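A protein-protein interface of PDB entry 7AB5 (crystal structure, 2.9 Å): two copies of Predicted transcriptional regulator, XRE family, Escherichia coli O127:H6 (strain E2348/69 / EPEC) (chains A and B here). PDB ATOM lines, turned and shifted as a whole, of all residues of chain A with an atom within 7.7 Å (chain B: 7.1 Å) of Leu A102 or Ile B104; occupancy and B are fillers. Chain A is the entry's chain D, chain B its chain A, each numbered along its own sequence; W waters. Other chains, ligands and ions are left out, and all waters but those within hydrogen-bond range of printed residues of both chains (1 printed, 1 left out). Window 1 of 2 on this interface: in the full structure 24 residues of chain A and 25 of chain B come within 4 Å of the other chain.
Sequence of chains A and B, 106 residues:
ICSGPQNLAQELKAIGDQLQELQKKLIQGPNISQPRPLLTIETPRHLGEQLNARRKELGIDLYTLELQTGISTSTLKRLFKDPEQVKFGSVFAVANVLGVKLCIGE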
ATOM      1  N   PRO A  37      -7.300   3.819  36.525  1.00  0.00           N
ATOM      2  CA  PRO A  37      -8.068   5.067  36.593  1.00  0.00           C
ATOM      3  C   PRO A  37      -8.774   5.371  35.276  1.00  0.00           C
ATOM      4  O   PRO A  37      -8.249   6.095  34.429  1.00  0.00           O
ATOM      5  CB  PRO A  37      -6.998   6.110  36.908  1.00  0.00           C
ATOM      6  CG  PRO A  37      -6.004   5.354  37.731  1.00  0.00           C
ATOM      7  CD  PRO A  37      -5.976   3.955  37.160  1.00  0.00           C
ATOM      8  N   LEU A  38      -9.974   4.816  35.127  1.00  0.00           N
ATOM      9  CA  LEU A  38     -10.719   4.832  33.878  1.00  0.00           C
ATOM     10  C   LEU A  38     -12.090   5.445  34.125  1.00  0.00           C
ATOM     11  O   LEU A  38     -12.762   5.091  35.098  1.00  0.00           O
ATOM     12  CB  LEU A  38     -10.853   3.408  33.331  1.00  0.00           C
ATOM     13  CG  LEU A  38     -11.784   3.115  32.160  1.00  0.00           C
ATOM     14  CD1 LEU A  38     -10.982   3.133  30.874  1.00  0.00           C
ATOM     15  CD2 LEU A  38     -12.465   1.771  32.358  1.00  0.00           C
ATOM     16  N   LEU A  39     -12.504   6.359  33.248  1.00  0.00           N
ATOM     17  CA  LEU A  39     -13.774   7.063  33.394  1.00  0.00           C
ATOM     18  C   LEU A  39     -14.509   7.043  32.061  1.00  0.00           C
ATOM     19  O   LEU A  39     -13.979   7.513  31.050  1.00  0.00           O
ATOM     20  CB  LEU A  39     -13.554   8.502  33.871  1.00  0.00           C
ATOM     21  CG  LEU A  39     -14.690   9.495  33.630  1.00  0.00           C
ATOM     22  CD1 LEU A  39     -15.773   9.332  34.684  1.00  0.00           C
ATOM     23  CD2 LEU A  39     -14.155  10.914  33.628  1.00  0.00           C
ATOM     24  N   THR A  40     -15.730   6.509  32.067  1.00  0.00           N
ATOM     25  CA  THR A  40     -16.509   6.351  30.845  1.00  0.00           C
ATOM     26  C   THR A  40     -17.260   7.642  30.540  1.00  0.00           C
ATOM     27  O   THR A  40     -18.016   8.142  31.381  1.00  0.00           O
ATOM     28  CB  THR A  40     -17.482   5.182  30.985  1.00  0.00           C
ATOM     29  OG1 THR A  40     -16.882   4.152  31.780  1.00  0.00           O
ATOM     30  CG2 THR A  40     -17.836   4.615  29.620  1.00  0.00           C
ATOM     31  N   ILE A  41     -17.060   8.172  29.334  1.00  0.00           N
ATOM     32  CA  ILE A  41     -17.692   9.425  28.932  1.00  0.00           C
ATOM     33  C   ILE A  41     -19.179   9.184  28.700  1.00  0.00           C
ATOM     34  O   ILE A  41     -19.568   8.362  27.862  1.00  0.00           O
ATOM     35  CB  ILE A  41     -17.018  10.001  27.680  1.00  0.00           C
ATOM     36  CG1 ILE A  41     -15.556  10.344  27.974  1.00  0.00           C
ATOM     37  CG2 ILE A  41     -17.765  11.228  27.188  1.00  0.00           C
ATOM     38  CD1 ILE A  41     -15.363  11.190  29.212  1.00  0.00           C
ATOM     39  N   HIS A  46     -19.922  15.922  29.358  1.00  0.00           N
ATOM     40  CA  HIS A  46     -19.094  15.240  30.348  1.00  0.00           C
ATOM     41  C   HIS A  46     -17.617  15.330  29.984  1.00  0.00           C
ATOM     42  O   HIS A  46     -16.778  15.678  30.822  1.00  0.00           O
ATOM     43  CB  HIS A  46     -19.541  13.782  30.464  1.00  0.00           C
ATOM     44  CG  HIS A  46     -18.960  13.050  31.632  1.00  0.00           C
ATOM     45  ND1 HIS A  46     -18.923  11.674  31.697  1.00  0.00           N
ATOM     46  CD2 HIS A  46     -18.404  13.497  32.782  1.00  0.00           C
ATOM     47  CE1 HIS A  46     -18.363  11.304  32.834  1.00  0.00           C
ATOM     48  NE2 HIS A  46     -18.039  12.391  33.511  1.00  0.00           N
ATOM     49  N   LEU A  47     -17.282  15.025  28.726  1.00  0.00           N
ATOM     50  CA  LEU A  47     -15.892  15.101  28.288  1.00  0.00           C
ATOM     51  C   LEU A  47     -15.371  16.530  28.365  1.00  0.00           C
ATOM     52  O   LEU A  47     -14.256  16.772  28.841  1.00  0.00           O
ATOM     53  CB  LEU A  47     -15.760  14.553  26.865  1.00  0.00           C
ATOM     54  CG  LEU A  47     -14.354  14.457  26.265  1.00  0.00           C
ATOM     55  CD1 LEU A  47     -13.329  14.023  27.303  1.00  0.00           C
ATOM     56  CD2 LEU A  47     -14.345  13.507  25.081  1.00  0.00           C
ATOM     57  N   GLN A  50     -14.661  17.354  32.024  1.00  0.00           N
ATOM     58  CA  GLN A  50     -13.459  16.709  32.542  1.00  0.00           C
ATOM     59  C   GLN A  50     -12.199  17.379  32.007  1.00  0.00           C
ATOM     60  O   GLN A  50     -11.254  17.638  32.761  1.00  0.00           O
ATOM     61  CB  GLN A  50     -13.464  15.221  32.194  1.00  0.00           C
ATOM     62  CG  GLN A  50     -14.549  14.419  32.886  1.00  0.00           C
ATOM     63  CD  GLN A  50     -14.411  14.438  34.394  1.00  0.00           C
ATOM     64  OE1 GLN A  50     -15.298  14.912  35.104  1.00  0.00           O
ATOM     65  NE2 GLN A  50     -13.290  13.929  34.893  1.00  0.00           N
ATOM     66  N   LEU A  51     -12.168  17.665  30.702  1.00  0.00           N
ATOM     67  CA  LEU A  51     -10.979  18.265  30.102  1.00  0.00           C
ATOM     68  C   LEU A  51     -10.700  19.645  30.681  1.00  0.00           C
ATOM     69  O   LEU A  51      -9.544  19.987  30.958  1.00  0.00           O
ATOM     70  CB  LEU A  51     -11.137  18.344  28.583  1.00  0.00           C
ATOM     71  CG  LEU A  51     -11.262  17.020  27.827  1.00  0.00           C
ATOM     72  CD1 LEU A  51     -11.391  17.268  26.331  1.00  0.00           C
ATOM     73  CD2 LEU A  51     -10.084  16.104  28.131  1.00  0.00           C
ATOM     74  N   ARG A  54      -9.297  19.053  34.031  1.00  0.00           N
ATOM     75  CA  ARG A  54      -7.902  18.649  33.879  1.00  0.00           C
ATOM     76  C   ARG A  54      -7.015  19.852  33.586  1.00  0.00           C
ATOM     77  O   ARG A  54      -5.938  20.006  34.173  1.00  0.00           O
ATOM     78  CB  ARG A  54      -7.784  17.613  32.762  1.00  0.00           C
ATOM     79  CG  ARG A  54      -6.362  17.357  32.308  1.00  0.00           C
ATOM     80  CD  ARG A  54      -5.649  16.455  33.293  1.00  0.00           C
ATOM     81  NE  ARG A  54      -4.360  15.998  32.791  1.00  0.00           N
ATOM     82  CZ  ARG A  54      -3.388  15.525  33.559  1.00  0.00           C
ATOM     83  NH1 ARG A  54      -3.530  15.431  34.871  1.00  0.00           N
ATOM     84  NH2 ARG A  54      -2.248  15.134  32.997  1.00  0.00           N
ATOM     85  N   PHE A  88     -14.180  16.826  15.873  1.00  0.00           N
ATOM     86  CA  PHE A  88     -13.586  15.766  16.682  1.00  0.00           C
ATOM     87  C   PHE A  88     -12.075  15.928  16.786  1.00  0.00           C
ATOM     88  O   PHE A  88     -11.485  15.637  17.833  1.00  0.00           O
ATOM     89  CB  PHE A  88     -13.933  14.396  16.102  1.00  0.00           C
ATOM     90  CG  PHE A  88     -13.309  13.253  16.846  1.00  0.00           C
ATOM     91  CD1 PHE A  88     -13.943  12.694  17.942  1.00  0.00           C
ATOM     92  CD2 PHE A  88     -12.081  12.743  16.458  1.00  0.00           C
ATOM     93  CE1 PHE A  88     -13.366  11.646  18.633  1.00  0.00           C
ATOM     94  CE2 PHE A  88     -11.498  11.699  17.145  1.00  0.00           C
ATOM     95  CZ  PHE A  88     -12.140  11.151  18.235  1.00  0.00           C
ATOM     96  N   VAL A  91     -11.135  18.292  19.721  1.00  0.00           N
ATOM     97  CA  VAL A  91     -11.303  17.640  21.018  1.00  0.00           C
ATOM     98  C   VAL A  91     -10.191  16.624  21.241  1.00  0.00           C
ATOM     99  O   VAL A  91      -9.579  16.570  22.315  1.00  0.00           O
ATOM    100  CB  VAL A  91     -12.692  16.986  21.116  1.00  0.00           C
ATOM    101  CG1 VAL A  91     -12.842  16.260  22.446  1.00  0.00           C
ATOM    102  CG2 VAL A  91     -13.782  18.032  20.949  1.00  0.00           C
ATOM    103  N   PHE A  92      -9.907  15.810  20.222  1.00  0.00           N
ATOM    104  CA  PHE A  92      -8.809  14.856  20.325  1.00  0.00           C
ATOM    105  C   PHE A  92      -7.471  15.564  20.502  1.00  0.00           C
ATOM    106  O   PHE A  92      -6.589  15.053  21.201  1.00  0.00           O
ATOM    107  CB  PHE A  92      -8.774  13.959  19.087  1.00  0.00           C
ATOM    108  CG  PHE A  92      -7.825  12.804  19.207  1.00  0.00           C
ATOM    109  CD1 PHE A  92      -8.206  11.642  19.857  1.00  0.00           C
ATOM    110  CD2 PHE A  92      -6.546  12.884  18.681  1.00  0.00           C
ATOM    111  CE1 PHE A  92      -7.332  10.578  19.973  1.00  0.00           C
ATOM    112  CE2 PHE A  92      -5.668  11.823  18.794  1.00  0.00           C
ATOM    113  CZ  PHE A  92      -6.062  10.670  19.441  1.00  0.00           C
ATOM    114  N   ALA A  95      -7.314  16.932  24.150  1.00  0.00           N
ATOM    115  CA  ALA A  95      -7.088  15.834  25.086  1.00  0.00           C
ATOM    116  C   ALA A  95      -5.619  15.428  25.118  1.00  0.00           C
ATOM    117  O   ALA A  95      -5.079  15.103  26.182  1.00  0.00           O
ATOM    118  CB  ALA A  95      -7.965  14.639  24.715  1.00  0.00           C
ATOM    119  N   ASN A  96      -4.951  15.447  23.962  1.00  0.00           N
ATOM    120  CA  ASN A  96      -3.556  15.021  23.903  1.00  0.00           C
ATOM    121  C   ASN A  96      -2.637  16.052  24.546  1.00  0.00           C
ATOM    122  O   ASN A  96      -1.766  15.703  25.353  1.00  0.00           O
ATOM    123  CB  ASN A  96      -3.144  14.762  22.455  1.00  0.00           C
ATOM    124  CG  ASN A  96      -3.243  13.300  22.078  1.00  0.00           C
ATOM    125  OD1 ASN A  96      -3.872  12.509  22.781  1.00  0.00           O
ATOM    126  ND2 ASN A  96      -2.613  12.929  20.970  1.00  0.00           N
ATOM    127  N   GLY A  99      -2.591  15.595  28.106  1.00  0.00           N
ATOM    128  CA  GLY A  99      -2.170  14.317  28.643  1.00  0.00           C
ATOM    129  C   GLY A  99      -3.284  13.327  28.883  1.00  0.00           C
ATOM    130  O   GLY A  99      -3.112  12.399  29.678  1.00  0.00           O
ATOM    131  N   VAL A 100      -4.425  13.492  28.219  1.00  0.00           N
ATOM    132  CA  VAL A 100      -5.571  12.604  28.374  1.00  0.00           C
ATOM    133  C   VAL A 100      -5.581  11.616  27.216  1.00  0.00           C
ATOM    134  O   VAL A 100      -5.400  12.004  26.055  1.00  0.00           O
ATOM    135  CB  VAL A 100      -6.888  13.398  28.427  1.00  0.00           C
ATOM    136  CG1 VAL A 100      -8.030  12.503  28.884  1.00  0.00           C
ATOM    137  CG2 VAL A 100      -6.745  14.603  29.342  1.00  0.00           C
ATOM    138  N   LYS A 101      -5.794  10.342  27.529  1.00  0.00           N
ATOM    139  CA  LYS A 101      -5.891   9.299  26.518  1.00  0.00           C
ATOM    140  C   LYS A 101      -7.343   8.882  26.331  1.00  0.00           C
ATOM    141  O   LYS A 101      -8.105   8.792  27.298  1.00  0.00           O
ATOM    142  CB  LYS A 101      -5.038   8.086  26.893  1.00  0.00           C
ATOM    143  CG  LYS A 101      -3.559   8.275  26.596  1.00  0.00           C
ATOM    144  CD  LYS A 101      -2.696   7.211  27.256  1.00  0.00           C
ATOM    145  CE  LYS A 101      -1.252   7.323  26.788  1.00  0.00           C
ATOM    146  NZ  LYS A 101      -0.648   5.994  26.493  1.00  0.00           N
ATOM    147  N   LEU A 102      -7.719   8.637  25.080  1.00  0.00           N
ATOM    148  CA  LEU A 102      -9.064   8.215  24.717  1.00  0.00           C
ATOM    149  C   LEU A 102      -9.062   6.711  24.474  1.00  0.00           C
ATOM    150  O   LEU A 102      -8.179   6.194  23.782  1.00  0.00           O
ATOM    151  CB  LEU A 102      -9.538   8.954  23.463  1.00  0.00           C
ATOM    152  CG  LEU A 102     -10.917   9.615  23.425  1.00  0.00           C
ATOM    153  CD1 LEU A 102     -11.032  10.692  24.485  1.00  0.00           C
ATOM    154  CD2 LEU A 102     -11.175  10.201  22.047  1.00  0.00           C
ATOM    155  N   CYS A 103     -10.041   6.015  25.046  1.00  0.00           N
ATOM    156  CA  CYS A 103     -10.161   4.572  24.895  1.00  0.00           C
ATOM    157  C   CYS A 103     -11.583   4.224  24.479  1.00  0.00           C
ATOM    158  O   CYS A 103     -12.506   5.030  24.621  1.00  0.00           O
ATOM    159  CB  CYS A 103      -9.803   3.833  26.195  1.00  0.00           C
ATOM    160  SG  CYS A 103      -8.456   4.578  27.146  1.00  0.00           S
ATOM    161  N   ILE A 104     -11.755   3.012  23.952  1.00  0.00           N
ATOM    162  CA  ILE A 104     -13.077   2.485  23.630  1.00  0.00           C
ATOM    163  C   ILE A 104     -13.185   1.049  24.127  1.00  0.00           C
ATOM    164  O   ILE A 104     -12.236   0.266  24.021  1.00  0.00           O
ATOM    165  CB  ILE A 104     -13.401   2.578  22.119  1.00  0.00           C
ATOM    166  CG1 ILE A 104     -12.512   1.649  21.290  1.00  0.00           C
ATOM    167  CG2 ILE A 104     -13.327   4.020  21.630  1.00  0.00           C
ATOM    168  CD1 ILE A 104     -12.911   1.581  19.830  1.00  0.00           C
ATOM    169  N   LEU B  39      -9.137  -0.377  24.044  1.00  0.00           N
ATOM    170  CA  LEU B  39      -8.272   0.000  22.933  1.00  0.00           C
ATOM    171  C   LEU B  39      -8.035   1.503  22.982  1.00  0.00           C
ATOM    172  O   LEU B  39      -8.989   2.287  22.966  1.00  0.00           O
ATOM    173  CB  LEU B  39      -8.892  -0.410  21.595  1.00  0.00           C
ATOM    174  CG  LEU B  39      -8.229   0.118  20.320  1.00  0.00           C
ATOM    175  CD1 LEU B  39      -6.735  -0.171  20.314  1.00  0.00           C
ATOM    176  CD2 LEU B  39      -8.893  -0.480  19.092  1.00  0.00           C
ATOM    177  N   THR B  40      -6.766   1.898  23.038  1.00  0.00           N
ATOM    178  CA  THR B  40      -6.402   3.309  23.068  1.00  0.00           C
ATOM    179  C   THR B  40      -6.485   3.886  21.660  1.00  0.00           C
ATOM    180  O   THR B  40      -5.844   3.375  20.735  1.00  0.00           O
ATOM    181  CB  THR B  40      -4.997   3.490  23.637  1.00  0.00           C
ATOM    182  OG1 THR B  40      -4.858   2.712  24.832  1.00  0.00           O
ATOM    183  CG2 THR B  40      -4.735   4.952  23.957  1.00  0.00           C
ATOM    184  N   ILE B  41      -7.272   4.947  21.499  1.00  0.00           N
ATOM    185  CA  ILE B  41      -7.392   5.609  20.205  1.00  0.00           C
ATOM    186  C   ILE B  41      -6.124   6.411  19.947  1.00  0.00           C
ATOM    187  O   ILE B  41      -5.818   7.364  20.673  1.00  0.00           O
ATOM    188  CB  ILE B  41      -8.638   6.501  20.159  1.00  0.00           C
ATOM    189  CG1 ILE B  41      -9.839   5.760  20.744  1.00  0.00           C
ATOM    190  CG2 ILE B  41      -8.934   6.930  18.737  1.00  0.00           C
ATOM    191  CD1 ILE B  41     -10.147   4.460  20.031  1.00  0.00           C
ATOM    192  N   GLU B  42      -5.378   6.025  18.910  1.00  0.00           N
ATOM    193  CA  GLU B  42      -4.116   6.697  18.612  1.00  0.00           C
ATOM    194  C   GLU B  42      -4.333   7.967  17.800  1.00  0.00           C
ATOM    195  O   GLU B  42      -3.694   8.992  18.063  1.00  0.00           O
ATOM    196  CB  GLU B  42      -3.176   5.752  17.861  1.00  0.00           C
ATOM    197  CG  GLU B  42      -3.378   4.280  18.172  1.00  0.00           C
ATOM    198  CD  GLU B  42      -2.619   3.830  19.400  1.00  0.00           C
ATOM    199  OE1 GLU B  42      -3.043   2.840  20.034  1.00  0.00           O
ATOM    200  OE2 GLU B  42      -1.596   4.467  19.733  1.00  0.00           O
ATOM    201  N   LEU B  47     -10.007   5.811  15.258  1.00  0.00           N
ATOM    202  CA  LEU B  47     -11.360   5.650  15.779  1.00  0.00           C
ATOM    203  C   LEU B  47     -12.346   5.300  14.672  1.00  0.00           C
ATOM    204  O   LEU B  47     -13.196   4.420  14.849  1.00  0.00           O
ATOM    205  CB  LEU B  47     -11.807   6.917  16.503  1.00  0.00           C
ATOM    206  CG  LEU B  47     -13.189   6.806  17.151  1.00  0.00           C
ATOM    207  CD1 LEU B  47     -13.250   5.602  18.077  1.00  0.00           C
ATOM    208  CD2 LEU B  47     -13.546   8.070  17.901  1.00  0.00           C
ATOM    209  N   PHE B  88     -17.908  16.414  16.982  1.00  0.00           N
ATOM    210  CA  PHE B  88     -17.684  15.392  17.999  1.00  0.00           C
ATOM    211  C   PHE B  88     -18.990  14.735  18.425  1.00  0.00           C
ATOM    212  O   PHE B  88     -19.022  13.533  18.716  1.00  0.00           O
ATOM    213  CB  PHE B  88     -16.973  15.996  19.210  1.00  0.00           C
ATOM    214  CG  PHE B  88     -16.890  15.065  20.384  1.00  0.00           C
ATOM    215  CD1 PHE B  88     -15.896  14.104  20.452  1.00  0.00           C
ATOM    216  CD2 PHE B  88     -17.810  15.145  21.417  1.00  0.00           C
ATOM    217  CE1 PHE B  88     -15.819  13.241  21.531  1.00  0.00           C
ATOM    218  CE2 PHE B  88     -17.739  14.283  22.496  1.00  0.00           C
ATOM    219  CZ  PHE B  88     -16.744  13.331  22.553  1.00  0.00           C
ATOM    220  N   LEU B 102     -17.014   4.837  25.302  1.00  0.00           N
ATOM    221  CA  LEU B 102     -15.905   5.770  25.136  1.00  0.00           C
ATOM    222  C   LEU B 102     -15.427   6.212  26.511  1.00  0.00           C
ATOM    223  O   LEU B 102     -16.180   6.841  27.262  1.00  0.00           O
ATOM    224  CB  LEU B 102     -16.323   6.975  24.294  1.00  0.00           C
ATOM    225  CG  LEU B 102     -15.201   7.717  23.569  1.00  0.00           C
ATOM    226  CD1 LEU B 102     -15.644   8.116  22.172  1.00  0.00           C
ATOM    227  CD2 LEU B 102     -14.762   8.937  24.366  1.00  0.00           C
ATOM    228  N   CYS B 103     -14.178   5.889  26.834  1.00  0.00           N
ATOM    229  CA  CYS B 103     -13.600   6.190  28.133  1.00  0.00           C
ATOM    230  C   CYS B 103     -12.368   7.067  27.956  1.00  0.00           C
ATOM    231  O   CYS B 103     -11.825   7.193  26.857  1.00  0.00           O
ATOM    232  CB  CYS B 103     -13.220   4.907  28.878  1.00  0.00           C
ATOM    233  SG  CYS B 103     -14.028   3.407  28.263  1.00  0.00           S
ATOM    234  N   ILE B 104     -11.929   7.679  29.054  1.00  0.00           N
ATOM    235  CA  ILE B 104     -10.712   8.480  29.062  1.00  0.00           C
ATOM    236  C   ILE B 104      -9.834   8.030  30.218  1.00  0.00           C
ATOM    237  O   ILE B 104     -10.327   7.739  31.314  1.00  0.00           O
ATOM    238  CB  ILE B 104     -11.000   9.996  29.157  1.00  0.00           C
ATOM    239  CG1 ILE B 104     -11.833  10.336  30.395  1.00  0.00           C
ATOM    240  CG2 ILE B 104     -11.704  10.487  27.914  1.00  0.00           C
ATOM    241  CD1 ILE B 104     -11.650  11.766  30.868  1.00  0.00           C
ATOM    242  N   GLY B 105      -8.528   7.963  29.962  1.00  0.00           N
ATOM    243  CA  GLY B 105      -7.557   7.644  30.985  1.00  0.00           C
ATOM    244  C   GLY B 105      -6.374   8.594  30.914  1.00  0.00           C
ATOM    245  O   GLY B 105      -6.361   9.547  30.133  1.00  0.00           O
ATOM    246  N   GLU B 106      -5.383   8.305  31.749  1.00  0.00           N
ATOM    247  CA  GLU B 106      -4.192   9.143  31.842  1.00  0.00           C
ATOM    248  C   GLU B 106      -2.931   8.293  31.946  1.00  0.00           C
ATOM    249  O   GLU B 106      -2.634   7.496  31.060  1.00  0.00           O
ATOM    250  CB  GLU B 106      -4.298  10.085  33.044  1.00  0.00           C
ATOM    251  CG  GLU B 106      -5.288  11.224  32.848  1.00  0.00           C
ATOM    252  CD  GLU B 106      -6.268  11.345  33.998  1.00  0.00           C
ATOM    253  OE1 GLU B 106      -5.858  11.111  35.155  1.00  0.00           O
ATOM    254  OE2 GLU B 106      -7.446  11.673  33.744  1.00  0.00           O
HETATM  255  O   HOH W   1      -5.892   9.673  22.968  1.00  0.00           O
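The backbone NH (N) of Ile A104 sits at hydrogen-bond distance from the backbone carbonyl oxygen (O) of Leu B39, at 3.0 Å.
O of Cys B103 is in hydrogen-bond range of N of Cys A103 (2.8 Å).
O of Gly B105 sits at hydrogen-bond distance from N of Lys A101.
The backbone NH (N) of Ile B41 is in hydrogen-bond range of the backbone carbonyl oxygen (O) of Leu A102, at 2.8 Å.
The backbone carbonyl oxygen of Leu A39 sits at hydrogen-bond distance from the backbone NH of Ile B104.
The backbone carbonyl oxygen (O) of Leu B102 is in hydrogen-bond range of the backbone NH (N) of Ile A41 (2.6 Å).
The backbone NH of Val A100 is in hydrogen-bond range of the backbone carbonyl oxygen of Ala A95, at 2.7 Å.
Leu A38 touches Ile B104.
Thr A40 touches Leu B102 (C to O, 3.5 Å).
Ile B104 touches Ile A41.
CD2 of Leu A47 touches CZ of Phe B88, at 3.5 Å.
CD1 of Leu A47 touches CG2 of Ile B104, at 3.9 Å.
Phe A88 touches Leu B47 (CZ to CD2, 3.4 Å).
Val A100 touches Gly B105.
CD of Lys A101 touches O of Glu B106, at 3.8 Å.
CA of Cys A103 touches O of Leu B39 (3.2 Å).
Ile A104 touches Ile B41 (CG2 to CD1, 3.6 Å).
Printed residues of chain B within 4 Å of Leu A47: Phe B88 and Ile B104.
Ala A95 touches none of the printed residues of chain B.
Gly A99 touches none of the printed residues of chain B.
Of the printed residues of chain B, Leu A102 touches Thr B40 (3.5 Å), Ile B41 (2.8 Å), Cys B103 (3.6 Å) and Ile B104 (3.5 Å).
Printed residues of chain A within 4 Å of Ile B41: Phe A92 (3.5 Å), Leu A102 (2.8 Å) and Ile A104 (3.6 Å).
Ile B104 touches just these residues of chain A: Leu A38 (3.9 Å), Leu A39 (2.9 Å), Ile A41 (3.8 Å), Leu A47 (3.9 Å), Val A100 (3.9 Å), Lys A101 (3.2 Å) and Leu A102 (3.5 Å).
Of the printed residues of chain A, Gly B105 touches Pro A37 (3.8 Å), Val A100 (3.6 Å) and Lys A101 (2.8 Å).
Printed residues of chain A within 4 Å of Glu B106: Lys A101 (3.8 Å).
The nearest printed residue of chain B that does not touch Leu A102 is Leu B102 (4.02 Å).
The nearest residue of chain A that does not touch Ile B104 is Pro A37 (4.1 Å).
Hydrophobic or aromatic side chains of chain A that line the printed part of chain B: Leu A38, Leu A39, Ile A41, Leu A47, Phe A88, Phe A92, Val A100, Leu A102 and Ile A104.
Printed residues of chain B that touch a printed residue of chain A: Leu B39, Thr B40, Ile B41, Glu B42, Leu B47, Phe B88, Leu B102, Cys B103, Ile B104, Gly B105 and Glu B106.
Among the printed residues, 30 pairs touch across the chains.
Among the printed residues, no Asp or Glu carboxylate lies within 4 Å of a Lys or Arg side-chain nitrogen of the other chain.
Leu A39 touches Cys B103, and with the chains exchanged Cys A103 touches Leu B39.
Leu A47 touches Phe B88, and with the chains exchanged Phe A88 touches Leu B47.
Leu A47 touches Ile B104, and with the chains exchanged Ile A104 touches Leu B47.
Phe B88 touches its own counterpart, Phe A88.
8 positions are printed for both chains.
Of the 30 pairs that touch across the chains among the printed residues, 18 have their exchanged pair printed and touching as well.
Water W1 lies within hydrogen-bond range of the backbone NH of Leu A102, the backbone carbonyl oxygen of Ile B41 and the side-chain amide oxygen of Asn A96.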
